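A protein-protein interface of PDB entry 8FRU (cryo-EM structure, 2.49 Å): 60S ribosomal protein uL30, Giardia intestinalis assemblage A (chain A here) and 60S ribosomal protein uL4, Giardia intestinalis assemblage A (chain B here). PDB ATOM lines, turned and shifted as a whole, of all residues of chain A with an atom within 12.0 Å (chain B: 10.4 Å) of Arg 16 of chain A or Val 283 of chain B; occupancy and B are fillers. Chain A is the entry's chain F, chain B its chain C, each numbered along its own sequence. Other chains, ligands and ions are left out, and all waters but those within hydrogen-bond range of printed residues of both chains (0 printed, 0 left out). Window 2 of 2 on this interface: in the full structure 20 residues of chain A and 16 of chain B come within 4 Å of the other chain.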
ATOM      1  N   GLN A  15     -14.978  -7.169 -22.094  1.00  0.00           N
ATOM      2  CA  GLN A  15     -15.034  -5.714 -22.182  1.00  0.00           C
ATOM      3  C   GLN A  15     -14.255  -5.060 -21.043  1.00  0.00           C
ATOM      4  O   GLN A  15     -14.462  -5.369 -19.870  1.00  0.00           O
ATOM      5  CB  GLN A  15     -16.488  -5.231 -22.185  1.00  0.00           C
ATOM      6  CG  GLN A  15     -17.430  -6.110 -22.994  1.00  0.00           C
ATOM      7  CD  GLN A  15     -17.995  -5.397 -24.214  1.00  0.00           C
ATOM      8  OE1 GLN A  15     -17.496  -4.349 -24.621  1.00  0.00           O
ATOM      9  NE2 GLN A  15     -19.039  -5.967 -24.803  1.00  0.00           N
ATOM     10  N   ARG A  16     -13.354  -4.154 -21.405  1.00  0.00           N
ATOM     11  CA  ARG A  16     -12.451  -3.503 -20.467  1.00  0.00           C
ATOM     12  C   ARG A  16     -12.790  -2.021 -20.395  1.00  0.00           C
ATOM     13  O   ARG A  16     -12.876  -1.352 -21.430  1.00  0.00           O
ATOM     14  CB  ARG A  16     -10.998  -3.699 -20.904  1.00  0.00           C
ATOM     15  CG  ARG A  16     -10.713  -5.075 -21.487  1.00  0.00           C
ATOM     16  CD  ARG A  16      -9.297  -5.552 -21.196  1.00  0.00           C
ATOM     17  NE  ARG A  16      -9.017  -5.659 -19.772  1.00  0.00           N
ATOM     18  CZ  ARG A  16      -9.178  -6.766 -19.062  1.00  0.00           C
ATOM     19  NH1 ARG A  16      -9.639  -7.878 -19.611  1.00  0.00           N
ATOM     20  NH2 ARG A  16      -8.870  -6.757 -17.770  1.00  0.00           N
ATOM     21  N   ASP A  17     -12.978  -1.510 -19.181  1.00  0.00           N
ATOM     22  CA  ASP A  17     -13.325  -0.110 -18.958  1.00  0.00           C
ATOM     23  C   ASP A  17     -12.109   0.653 -18.454  1.00  0.00           C
ATOM     24  O   ASP A  17     -11.353   0.148 -17.619  1.00  0.00           O
ATOM     25  CB  ASP A  17     -14.478   0.034 -17.962  1.00  0.00           C
ATOM     26  CG  ASP A  17     -15.810  -0.404 -18.541  1.00  0.00           C
ATOM     27  OD1 ASP A  17     -15.902  -0.552 -19.779  1.00  0.00           O
ATOM     28  OD2 ASP A  17     -16.777  -0.556 -17.762  1.00  0.00           O
ATOM     29  N   ILE A  18     -11.928   1.869 -18.959  1.00  0.00           N
ATOM     30  CA  ILE A  18     -10.749   2.667 -18.648  1.00  0.00           C
ATOM     31  C   ILE A  18     -11.032   3.622 -17.495  1.00  0.00           C
ATOM     32  O   ILE A  18     -10.115   4.022 -16.770  1.00  0.00           O
ATOM     33  CB  ILE A  18     -10.279   3.440 -19.891  1.00  0.00           C
ATOM     34  CG1 ILE A  18      -8.847   3.941 -19.704  1.00  0.00           C
ATOM     35  CG2 ILE A  18     -11.214   4.599 -20.165  1.00  0.00           C
ATOM     36  CD1 ILE A  18      -8.299   4.663 -20.912  1.00  0.00           C
ATOM     37  N   ARG A  19     -12.295   3.994 -17.318  1.00  0.00           N
ATOM     38  CA  ARG A  19     -12.647   5.004 -16.334  1.00  0.00           C
ATOM     39  C   ARG A  19     -12.569   4.445 -14.914  1.00  0.00           C
ATOM     40  O   ARG A  19     -12.672   3.239 -14.680  1.00  0.00           O
ATOM     41  CB  ARG A  19     -14.045   5.552 -16.610  1.00  0.00           C
ATOM     42  CG  ARG A  19     -14.145   6.346 -17.899  1.00  0.00           C
ATOM     43  CD  ARG A  19     -15.540   6.907 -18.100  1.00  0.00           C
ATOM     44  N   SER A  20     -12.393   5.355 -13.959  1.00  0.00           N
ATOM     45  CA  SER A  20     -12.223   5.011 -12.555  1.00  0.00           C
ATOM     46  C   SER A  20     -13.561   4.652 -11.912  1.00  0.00           C
ATOM     47  O   SER A  20     -14.629   4.754 -12.521  1.00  0.00           O
ATOM     48  CB  SER A  20     -11.559   6.164 -11.811  1.00  0.00           C
ATOM     49  OG  SER A  20     -11.585   5.943 -10.416  1.00  0.00           O
ATOM     50  N   ALA A  21     -13.500   4.232 -10.646  1.00  0.00           N
ATOM     51  CA  ALA A  21     -14.703   3.785  -9.953  1.00  0.00           C
ATOM     52  C   ALA A  21     -15.707   4.918  -9.760  1.00  0.00           C
ATOM     53  O   ALA A  21     -16.911   4.729  -9.972  1.00  0.00           O
ATOM     54  CB  ALA A  21     -14.329   3.168  -8.607  1.00  0.00           C
ATOM     55  N   ARG A  24     -17.678   5.779 -12.838  1.00  0.00           N
ATOM     56  CA  ARG A  24     -18.685   4.756 -13.087  1.00  0.00           C
ATOM     57  C   ARG A  24     -19.883   4.938 -12.170  1.00  0.00           C
ATOM     58  O   ARG A  24     -21.030   4.855 -12.618  1.00  0.00           O
ATOM     59  CB  ARG A  24     -18.086   3.361 -12.914  1.00  0.00           C
ATOM     60  CG  ARG A  24     -16.778   3.124 -13.661  1.00  0.00           C
ATOM     61  CD  ARG A  24     -16.360   1.662 -13.586  1.00  0.00           C
ATOM     62  NE  ARG A  24     -14.951   1.501 -13.247  1.00  0.00           N
ATOM     63  CZ  ARG A  24     -14.259   0.381 -13.414  1.00  0.00           C
ATOM     64  NH1 ARG A  24     -14.802  -0.696 -13.954  1.00  0.00           N
ATOM     65  NH2 ARG A  24     -12.986   0.343 -13.029  1.00  0.00           N
ATOM     66  N   VAL B 278       5.425  -4.490 -16.621  1.00  0.00           N
ATOM     67  CA  VAL B 278       4.293  -5.355 -16.923  1.00  0.00           C
ATOM     68  C   VAL B 278       2.987  -4.731 -16.454  1.00  0.00           C
ATOM     69  O   VAL B 278       1.926  -5.000 -17.026  1.00  0.00           O
ATOM     70  CB  VAL B 278       4.511  -6.743 -16.298  1.00  0.00           C
ATOM     71  CG1 VAL B 278       3.299  -7.625 -16.511  1.00  0.00           C
ATOM     72  CG2 VAL B 278       5.740  -7.392 -16.890  1.00  0.00           C
ATOM     73  N   GLN B 279       3.036  -3.890 -15.421  1.00  0.00           N
ATOM     74  CA  GLN B 279       1.813  -3.312 -14.876  1.00  0.00           C
ATOM     75  C   GLN B 279       1.230  -2.243 -15.788  1.00  0.00           C
ATOM     76  O   GLN B 279       0.018  -2.012 -15.771  1.00  0.00           O
ATOM     77  CB  GLN B 279       2.087  -2.732 -13.490  1.00  0.00           C
ATOM     78  CG  GLN B 279       2.327  -3.771 -12.413  1.00  0.00           C
ATOM     79  CD  GLN B 279       1.178  -4.743 -12.265  1.00  0.00           C
ATOM     80  OE1 GLN B 279       0.100  -4.535 -12.817  1.00  0.00           O
ATOM     81  NE2 GLN B 279       1.409  -5.823 -11.535  1.00  0.00           N
ATOM     82  N   LYS B 280       2.068  -1.580 -16.585  1.00  0.00           N
ATOM     83  CA  LYS B 280       1.579  -0.523 -17.460  1.00  0.00           C
ATOM     84  C   LYS B 280       0.563  -1.029 -18.472  1.00  0.00           C
ATOM     85  O   LYS B 280      -0.215  -0.230 -19.004  1.00  0.00           O
ATOM     86  CB  LYS B 280       2.741   0.135 -18.199  1.00  0.00           C
ATOM     87  CG  LYS B 280       3.997   0.291 -17.379  1.00  0.00           C
ATOM     88  CD  LYS B 280       4.925   1.317 -18.006  1.00  0.00           C
ATOM     89  CE  LYS B 280       5.833   1.954 -16.970  1.00  0.00           C
ATOM     90  NZ  LYS B 280       6.569   0.940 -16.169  1.00  0.00           N
ATOM     91  N   THR B 281       0.554  -2.325 -18.758  1.00  0.00           N
ATOM     92  CA  THR B 281      -0.337  -2.864 -19.774  1.00  0.00           C
ATOM     93  C   THR B 281      -1.693  -3.287 -19.226  1.00  0.00           C
ATOM     94  O   THR B 281      -2.584  -3.611 -20.016  1.00  0.00           O
ATOM     95  CB  THR B 281       0.324  -4.058 -20.469  1.00  0.00           C
ATOM     96  OG1 THR B 281       0.559  -5.099 -19.514  1.00  0.00           O
ATOM     97  CG2 THR B 281       1.645  -3.646 -21.089  1.00  0.00           C
ATOM     98  N   PHE B 282      -1.879  -3.280 -17.912  1.00  0.00           N
ATOM     99  CA  PHE B 282      -3.127  -3.757 -17.337  1.00  0.00           C
ATOM    100  C   PHE B 282      -4.244  -2.740 -17.541  1.00  0.00           C
ATOM    101  O   PHE B 282      -4.053  -1.536 -17.357  1.00  0.00           O
ATOM    102  CB  PHE B 282      -2.943  -4.050 -15.852  1.00  0.00           C
ATOM    103  CG  PHE B 282      -2.247  -5.347 -15.578  1.00  0.00           C
ATOM    104  CD1 PHE B 282      -1.481  -5.955 -16.555  1.00  0.00           C
ATOM    105  CD2 PHE B 282      -2.353  -5.959 -14.349  1.00  0.00           C
ATOM    106  CE1 PHE B 282      -0.836  -7.143 -16.310  1.00  0.00           C
ATOM    107  CE2 PHE B 282      -1.709  -7.149 -14.099  1.00  0.00           C
ATOM    108  CZ  PHE B 282      -0.951  -7.740 -15.081  1.00  0.00           C
ATOM    109  N   VAL B 283      -5.423  -3.238 -17.920  1.00  0.00           N
ATOM    110  CA  VAL B 283      -6.580  -2.406 -18.205  1.00  0.00           C
ATOM    111  C   VAL B 283      -7.768  -2.966 -17.435  1.00  0.00           C
ATOM    112  O   VAL B 283      -8.101  -4.144 -17.589  1.00  0.00           O
ATOM    113  CB  VAL B 283      -6.900  -2.349 -19.710  1.00  0.00           C
ATOM    114  CG1 VAL B 283      -8.153  -1.535 -19.954  1.00  0.00           C
ATOM    115  CG2 VAL B 283      -5.726  -1.775 -20.479  1.00  0.00           C
ATOM    116  N   PRO B 284      -8.445  -2.174 -16.607  1.00  0.00           N
ATOM    117  CA  PRO B 284      -9.522  -2.727 -15.776  1.00  0.00           C
ATOM    118  C   PRO B 284     -10.672  -3.259 -16.616  1.00  0.00           C
ATOM    119  O   PRO B 284     -10.991  -2.732 -17.682  1.00  0.00           O
ATOM    120  CB  PRO B 284      -9.966  -1.535 -14.920  1.00  0.00           C
ATOM    121  CG  PRO B 284      -8.919  -0.487 -15.107  1.00  0.00           C
ATOM    122  CD  PRO B 284      -8.322  -0.718 -16.451  1.00  0.00           C
ATOM    123  N   LYS B 285     -11.300  -4.314 -16.118  1.00  0.00           N
ATOM    124  CA  LYS B 285     -12.482  -4.869 -16.754  1.00  0.00           C
ATOM    125  C   LYS B 285     -13.737  -4.221 -16.186  1.00  0.00           C
ATOM    126  O   LYS B 285     -13.784  -3.828 -15.019  1.00  0.00           O
ATOM    127  CB  LYS B 285     -12.540  -6.383 -16.564  1.00  0.00           C
ATOM    128  CG  LYS B 285     -12.931  -6.816 -15.170  1.00  0.00           C
ATOM    129  CD  LYS B 285     -12.446  -8.224 -14.883  1.00  0.00           C
ATOM    130  CE  LYS B 285     -12.312  -9.031 -16.164  1.00  0.00           C
ATOM    131  NZ  LYS B 285     -12.466 -10.490 -15.916  1.00  0.00           N
ATOM    132  N   ARG B 286     -14.760  -4.118 -17.030  1.00  0.00           N
ATOM    133  CA  ARG B 286     -16.002  -3.472 -16.641  1.00  0.00           C
ATOM    134  C   ARG B 286     -16.603  -4.143 -15.411  1.00  0.00           C
ATOM    135  O   ARG B 286     -16.245  -5.263 -15.041  1.00  0.00           O
ATOM    136  CB  ARG B 286     -17.001  -3.510 -17.794  1.00  0.00           C
ATOM    137  CG  ARG B 286     -17.332  -4.912 -18.252  1.00  0.00           C
ATOM    138  CD  ARG B 286     -18.618  -4.950 -19.041  1.00  0.00           C
ATOM    139  NE  ARG B 286     -18.822  -6.247 -19.671  1.00  0.00           N
ATOM    140  CZ  ARG B 286     -19.865  -6.553 -20.430  1.00  0.00           C
ATOM    141  NH1 ARG B 286     -20.821  -5.672 -20.674  1.00  0.00           N
ATOM    142  NH2 ARG B 286     -19.953  -7.771 -20.954  1.00  0.00           N
ATOM    143  N   ASP B 287     -17.527  -3.436 -14.771  1.00  0.00           N
ATOM    144  CA  ASP B 287     -18.175  -3.969 -13.584  1.00  0.00           C
ATOM    145  C   ASP B 287     -19.103  -5.122 -13.963  1.00  0.00           C
ATOM    146  O   ASP B 287     -19.730  -5.092 -15.025  1.00  0.00           O
ATOM    147  CB  ASP B 287     -18.960  -2.876 -12.867  1.00  0.00           C
ATOM    148  CG  ASP B 287     -18.146  -2.190 -11.788  1.00  0.00           C
ATOM    149  OD1 ASP B 287     -18.059  -2.738 -10.671  1.00  0.00           O
ATOM    150  OD2 ASP B 287     -17.587  -1.107 -12.059  1.00  0.00           O
ATOM    151  N   PRO B 288     -19.217  -6.140 -13.117  1.00  0.00           N
ATOM    152  CA  PRO B 288     -19.983  -7.333 -13.488  1.00  0.00           C
ATOM    153  C   PRO B 288     -21.481  -7.078 -13.463  1.00  0.00           C
ATOM    154  O   PRO B 288     -21.968  -6.024 -13.052  1.00  0.00           O
ATOM    155  CB  PRO B 288     -19.575  -8.357 -12.427  1.00  0.00           C
ATOM    156  CG  PRO B 288     -19.184  -7.541 -11.253  1.00  0.00           C
ATOM    157  CD  PRO B 288     -18.581  -6.277 -11.796  1.00  0.00           C
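O of Gln 15 of chain A lies within hydrogen-bond range of N of Arg 286 of chain B, 3.1 Å away.
The guanidinium group (NH2) of Arg 16 of chain A lies within hydrogen-bond range of the backbone carbonyl oxygen (O) of Val 283 of chain B.
The backbone NH (N) of Asp 17 of chain A is in hydrogen-bond range of the backbone carbonyl oxygen (O) of Pro 284 of chain B (2.8 Å).
The guanidinium group (NH1) of Arg 24 of chain A is in hydrogen-bond range of the backbone carbonyl oxygen (O) of Lys 285 of chain B, 3.5 Å away.
NH1 of Arg 24 of chain A lies within salt-bridge range of OD2 of Asp 287 of chain B, at 3.4 Å.
O of Arg 19 of chain A sits at hydrogen-bond distance from NE of Arg 24 of chain A (3.2 Å).
The backbone carbonyl oxygen of Ser 20 of chain A lies close to the guanidinium group of Arg 24 of chain A, 3.3 Å away.
Among the printed residues, merely in contact across the chains: Asp 17 of chain A with Arg 286 of chain B (3.0 Å), Arg 16 of chain A with Pro 284 of chain B (3.2 Å), Gln 15 of chain A with Lys 285 of chain B (3.7 Å) and Arg 16 of chain A with Lys 285 of chain B (3.8 Å).
Arg 16 of chain A touches just these residues of chain B: Val 283 (2.7 Å), Pro 284 (3.2 Å) and Lys 285 (3.8 Å).
Of chain B, only Pro 284 and Arg 286 come within 4 Å of Asp 17 of chain A.
No residue of chain A comes within 4 Å of Thr 281 of chain B.
No residue of chain A comes within 4 Å of Phe 282 of chain B.
Of the printed residues of chain A, Lys 285 of chain B touches Gln 15, Arg 16 and Arg 24.
Arg 286 of chain B touches just these residues of chain A: Gln 15 (3.1 Å) and Asp 17 (3.0 Å).
Printed residues of chain B within 4 Å of Gln 15 of chain A: Lys 285 and Arg 286.
Printed residues of chain B within 4 Å of Arg 24 of chain A: Lys 285 and Asp 287.
Gln 279 of chain B touches none of the printed residues of chain A.
Ser 20 of chain A touches none of the printed residues of chain B.
The nearest residue of chain A that does not touch Val 283 of chain B is Asp 17 of chain A (4.3 Å).
The nearest printed residue of chain B that does not touch Arg 24 of chain A is Pro 284 of chain B (4.03 Å).
Of the 11 printed residues of chain B, 5 touch a printed residue of chain A.
Hydrophobic or aromatic side chains of chain B within 4 Å of the printed part of chain A: Val 283 and Pro 284.
Among the printed residues, 9 pairs touch across the chains.
Among the printed residues, Asp or Glu carboxylates within 4 Å of a Lys or Arg side-chain nitrogen of the other chain: Arg 24 of chain A with Asp 287 of chain B (3.4 Å).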
